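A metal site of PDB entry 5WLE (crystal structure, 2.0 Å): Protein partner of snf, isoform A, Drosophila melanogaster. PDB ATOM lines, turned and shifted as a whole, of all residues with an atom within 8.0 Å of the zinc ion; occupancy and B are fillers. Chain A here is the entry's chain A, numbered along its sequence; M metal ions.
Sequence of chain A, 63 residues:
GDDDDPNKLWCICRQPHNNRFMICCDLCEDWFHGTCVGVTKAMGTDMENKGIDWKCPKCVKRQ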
ATOM      1  N   CYS A  24      25.183   8.312   3.400  1.00  0.00           N
ATOM      2  CA  CYS A  24      24.401   7.417   2.541  1.00  0.00           C
ATOM      3  C   CYS A  24      24.686   7.764   1.087  1.00  0.00           C
ATOM      4  O   CYS A  24      24.487   8.904   0.670  1.00  0.00           O
ATOM      5  CB  CYS A  24      22.909   7.563   2.844  1.00  0.00           C
ATOM      6  SG  CYS A  24      21.827   6.325   2.133  1.00  0.00           S
ATOM      7  N   CYS A  25      25.143   6.780   0.316  1.00  0.00           N
ATOM      8  CA  CYS A  25      25.423   6.990  -1.103  1.00  0.00           C
ATOM      9  C   CYS A  25      24.146   7.307  -1.884  1.00  0.00           C
ATOM     10  O   CYS A  25      23.122   6.631  -1.748  1.00  0.00           O
ATOM     11  CB  CYS A  25      26.098   5.748  -1.693  1.00  0.00           C
ATOM     12  SG  CYS A  25      26.390   5.790  -3.471  1.00  0.00           S
ATOM     13  N   ASP A  26      24.218   8.305  -2.748  1.00  0.00           N
ATOM     14  CA  ASP A  26      23.003   8.687  -3.454  1.00  0.00           C
ATOM     15  C   ASP A  26      22.680   7.778  -4.640  1.00  0.00           C
ATOM     16  O   ASP A  26      21.660   8.008  -5.306  1.00  0.00           O
ATOM     17  CB  ASP A  26      23.091  10.150  -3.904  1.00  0.00           C
ATOM     18  CG  ASP A  26      22.827  11.125  -2.750  1.00  0.00           C
ATOM     19  OD1 ASP A  26      21.799  10.983  -2.050  1.00  0.00           O
ATOM     20  OD2 ASP A  26      23.666  12.010  -2.522  1.00  0.00           O
ATOM     21  N   LEU A  27      23.484   6.758  -4.935  1.00  0.00           N
ATOM     22  CA  LEU A  27      23.130   5.792  -5.976  1.00  0.00           C
ATOM     23  C   LEU A  27      22.780   4.420  -5.431  1.00  0.00           C
ATOM     24  O   LEU A  27      21.730   3.867  -5.798  1.00  0.00           O
ATOM     25  CB  LEU A  27      24.270   5.657  -7.005  1.00  0.00           C
ATOM     26  CG  LEU A  27      23.925   4.763  -8.204  1.00  0.00           C
ATOM     27  CD1 LEU A  27      22.613   5.195  -8.894  1.00  0.00           C
ATOM     28  CD2 LEU A  27      25.056   4.735  -9.218  1.00  0.00           C
ATOM     29  N   CYS A  28      23.613   3.834  -4.576  1.00  0.00           N
ATOM     30  CA  CYS A  28      23.258   2.529  -4.049  1.00  0.00           C
ATOM     31  C   CYS A  28      22.387   2.626  -2.807  1.00  0.00           C
ATOM     32  O   CYS A  28      21.717   1.636  -2.459  1.00  0.00           O
ATOM     33  CB  CYS A  28      24.520   1.686  -3.761  1.00  0.00           C
ATOM     34  SG  CYS A  28      25.657   2.308  -2.497  1.00  0.00           S
ATOM     35  N   GLU A  29      22.355   3.776  -2.143  1.00  0.00           N
ATOM     36  CA  GLU A  29      21.571   4.054  -0.941  1.00  0.00           C
ATOM     37  C   GLU A  29      22.074   3.279   0.260  1.00  0.00           C
ATOM     38  O   GLU A  29      21.379   3.192   1.278  1.00  0.00           O
ATOM     39  CB  GLU A  29      20.078   3.769  -1.163  1.00  0.00           C
ATOM     40  CG  GLU A  29      19.476   4.469  -2.389  1.00  0.00           C
ATOM     41  CD  GLU A  29      17.962   4.350  -2.451  1.00  0.00           C
ATOM     42  OE1 GLU A  29      17.462   3.224  -2.656  1.00  0.00           O
ATOM     43  OE2 GLU A  29      17.270   5.387  -2.277  1.00  0.00           O
ATOM     44  N   ASP A  30      23.256   2.693   0.174  1.00  0.00           N
ATOM     45  CA  ASP A  30      23.857   2.056   1.325  1.00  0.00           C
ATOM     46  C   ASP A  30      24.653   3.081   2.128  1.00  0.00           C
ATOM     47  O   ASP A  30      24.974   4.164   1.634  1.00  0.00           O
ATOM     48  CB  ASP A  30      24.758   0.901   0.889  1.00  0.00           C
ATOM     49  CG  ASP A  30      23.969  -0.342   0.554  1.00  0.00           C
ATOM     50  OD1 ASP A  30      22.821  -0.444   1.043  1.00  0.00           O
ATOM     51  OD2 ASP A  30      24.485  -1.200  -0.186  1.00  0.00           O
ATOM     52  N   TRP A  31      24.956   2.719   3.374  1.00  0.00           N
ATOM     53  CA  TRP A  31      25.613   3.608   4.320  1.00  0.00           C
ATOM     54  C   TRP A  31      27.090   3.261   4.472  1.00  0.00           C
ATOM     55  O   TRP A  31      27.463   2.079   4.495  1.00  0.00           O
ATOM     56  CB  TRP A  31      24.925   3.552   5.683  1.00  0.00           C
ATOM     57  CG  TRP A  31      23.574   4.158   5.692  1.00  0.00           C
ATOM     58  CD1 TRP A  31      22.382   3.531   5.436  1.00  0.00           C
ATOM     59  CD2 TRP A  31      23.260   5.525   5.999  1.00  0.00           C
ATOM     60  NE1 TRP A  31      21.350   4.435   5.546  1.00  0.00           N
ATOM     61  CE2 TRP A  31      21.855   5.655   5.910  1.00  0.00           C
ATOM     62  CE3 TRP A  31      24.016   6.645   6.349  1.00  0.00           C
ATOM     63  CZ2 TRP A  31      21.202   6.866   6.144  1.00  0.00           C
ATOM     64  CZ3 TRP A  31      23.363   7.857   6.584  1.00  0.00           C
ATOM     65  CH2 TRP A  31      21.968   7.952   6.482  1.00  0.00           C
ATOM     66  N   PHE A  32      27.913   4.291   4.624  1.00  0.00           N
ATOM     67  CA  PHE A  32      29.363   4.158   4.689  1.00  0.00           C
ATOM     68  C   PHE A  32      29.886   4.980   5.847  1.00  0.00           C
ATOM     69  O   PHE A  32      29.447   6.109   6.067  1.00  0.00           O
ATOM     70  CB  PHE A  32      29.995   4.612   3.357  1.00  0.00           C
ATOM     71  CG  PHE A  32      29.580   3.774   2.189  1.00  0.00           C
ATOM     72  CD1 PHE A  32      28.354   3.971   1.568  1.00  0.00           C
ATOM     73  CD2 PHE A  32      30.393   2.744   1.736  1.00  0.00           C
ATOM     74  CE1 PHE A  32      27.952   3.175   0.514  1.00  0.00           C
ATOM     75  CE2 PHE A  32      30.011   1.951   0.691  1.00  0.00           C
ATOM     76  CZ  PHE A  32      28.776   2.168   0.071  1.00  0.00           C
ATOM     77  N   TRP A  54      26.346  12.803  -3.223  1.00  0.00           N
ATOM     78  CA  TRP A  54      27.613  12.124  -3.022  1.00  0.00           C
ATOM     79  C   TRP A  54      27.448  10.643  -3.357  1.00  0.00           C
ATOM     80  O   TRP A  54      26.392  10.060  -3.058  1.00  0.00           O
ATOM     81  CB  TRP A  54      28.109  12.306  -1.573  1.00  0.00           C
ATOM     82  CG  TRP A  54      29.344  11.502  -1.247  1.00  0.00           C
ATOM     83  CD1 TRP A  54      30.646  11.878  -1.451  1.00  0.00           C
ATOM     84  CD2 TRP A  54      29.377  10.196  -0.667  1.00  0.00           C
ATOM     85  NE1 TRP A  54      31.486  10.877  -1.023  1.00  0.00           N
ATOM     86  CE2 TRP A  54      30.736   9.834  -0.543  1.00  0.00           C
ATOM     87  CE3 TRP A  54      28.398   9.297  -0.250  1.00  0.00           C
ATOM     88  CZ2 TRP A  54      31.121   8.611  -0.017  1.00  0.00           C
ATOM     89  CZ3 TRP A  54      28.797   8.085   0.274  1.00  0.00           C
ATOM     90  CH2 TRP A  54      30.147   7.749   0.384  1.00  0.00           C
ATOM     91  N   LYS A  55      28.454  10.064  -3.994  1.00  0.00           N
ATOM     92  CA  LYS A  55      28.476   8.646  -4.339  1.00  0.00           C
ATOM     93  C   LYS A  55      29.686   7.955  -3.736  1.00  0.00           C
ATOM     94  O   LYS A  55      30.780   8.532  -3.680  1.00  0.00           O
ATOM     95  CB  LYS A  55      28.504   8.447  -5.868  1.00  0.00           C
ATOM     96  CG  LYS A  55      27.179   8.750  -6.532  1.00  0.00           C
ATOM     97  CD  LYS A  55      27.120   8.138  -7.915  1.00  0.00           C
ATOM     98  CE  LYS A  55      27.492   9.140  -8.956  1.00  0.00           C
ATOM     99  NZ  LYS A  55      26.398  10.151  -9.047  1.00  0.00           N
ATOM    100  N   CYS A  56      29.488   6.710  -3.300  1.00  0.00           N
ATOM    101  CA  CYS A  56      30.553   5.909  -2.724  1.00  0.00           C
ATOM    102  C   CYS A  56      31.573   5.551  -3.820  1.00  0.00           C
ATOM    103  O   CYS A  56      31.296   5.731  -5.017  1.00  0.00           O
ATOM    104  CB  CYS A  56      29.966   4.667  -2.062  1.00  0.00           C
ATOM    105  SG  CYS A  56      29.503   3.385  -3.249  1.00  0.00           S
ATOM    106  N   PRO A  57      32.758   5.064  -3.456  1.00  0.00           N
ATOM    107  CA  PRO A  57      33.787   4.818  -4.486  1.00  0.00           C
ATOM    108  C   PRO A  57      33.352   3.796  -5.519  1.00  0.00           C
ATOM    109  O   PRO A  57      33.645   3.954  -6.711  1.00  0.00           O
ATOM    110  CB  PRO A  57      35.004   4.347  -3.684  1.00  0.00           C
ATOM    111  CG  PRO A  57      34.783   4.911  -2.294  1.00  0.00           C
ATOM    112  CD  PRO A  57      33.289   4.799  -2.100  1.00  0.00           C
ATOM    113  N   LYS A  58      32.647   2.752  -5.094  1.00  0.00           N
ATOM    114  CA  LYS A  58      32.192   1.741  -6.044  1.00  0.00           C
ATOM    115  C   LYS A  58      31.167   2.325  -7.015  1.00  0.00           C
ATOM    116  O   LYS A  58      31.219   2.058  -8.224  1.00  0.00           O
ATOM    117  CB  LYS A  58      31.611   0.544  -5.291  1.00  0.00           C
ATOM    118  CG  LYS A  58      30.972  -0.515  -6.183  1.00  0.00           C
ATOM    119  CD  LYS A  58      30.186  -1.516  -5.380  1.00  0.00           C
ATOM    120  CE  LYS A  58      28.949  -0.869  -4.778  1.00  0.00           C
ATOM    121  NZ  LYS A  58      28.159  -0.087  -5.805  1.00  0.00           N
ATOM    122  N   CYS A  59      30.248   3.135  -6.506  1.00  0.00           N
ATOM    123  CA  CYS A  59      29.259   3.734  -7.390  1.00  0.00           C
ATOM    124  C   CYS A  59      29.872   4.761  -8.323  1.00  0.00           C
ATOM    125  O   CYS A  59      29.401   4.926  -9.451  1.00  0.00           O
ATOM    126  CB  CYS A  59      28.126   4.364  -6.571  1.00  0.00           C
ATOM    127  SG  CYS A  59      26.921   3.116  -6.043  1.00  0.00           S
ATOM    128  N   VAL A  60      30.936   5.448  -7.887  1.00  0.00           N
ATOM    129  CA  VAL A  60      31.609   6.399  -8.767  1.00  0.00           C
ATOM    130  C   VAL A  60      32.196   5.686  -9.994  1.00  0.00           C
ATOM    131  O   VAL A  60      32.136   6.213 -11.112  1.00  0.00           O
ATOM    132  CB  VAL A  60      32.689   7.179  -7.988  1.00  0.00           C
ATOM    133  CG1 VAL A  60      33.674   7.841  -8.944  1.00  0.00           C
ATOM    134  CG2 VAL A  60      32.028   8.239  -7.114  1.00  0.00           C
HETATM  135 ZN    ZN M   1      27.172   3.611  -3.712  1.00  0.00          ZN
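The side-chain sulfur (SG) of Cys 25 lies close to the backbone NH (N) of Leu 27, 3.4 Å away. The backbone NH of Cys 25 sits at hydrogen-bond distance from the backbone carbonyl oxygen of Asp 30, at 2.9 Å. The side-chain sulfur (SG) of Cys 28 lies close to the backbone NH (N) of Asp 30 (3.6 Å). The side-chain sulfur (SG) of Cys 56 sits close to the backbone NH (N) of Lys 58 (3.7 Å). The side-chain amino group of Lys 58 sits close to the side-chain sulfur of Cys 59, 3.4 Å away.
SG of Cys 25 binds the zinc ion (2.3 Å). The zinc ion is bound by SG of Cys 28 (2.3 Å). The zinc ion is bound by SG of Cys 56 (2.4 Å). The zinc ion is bound by the side-chain sulfur (SG) of Cys 59 (2.4 Å). The zinc ion has four donor atoms within binding distance.
The nearest printed residue that does not touch the zinc ion is Phe 32 (4.3 Å).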
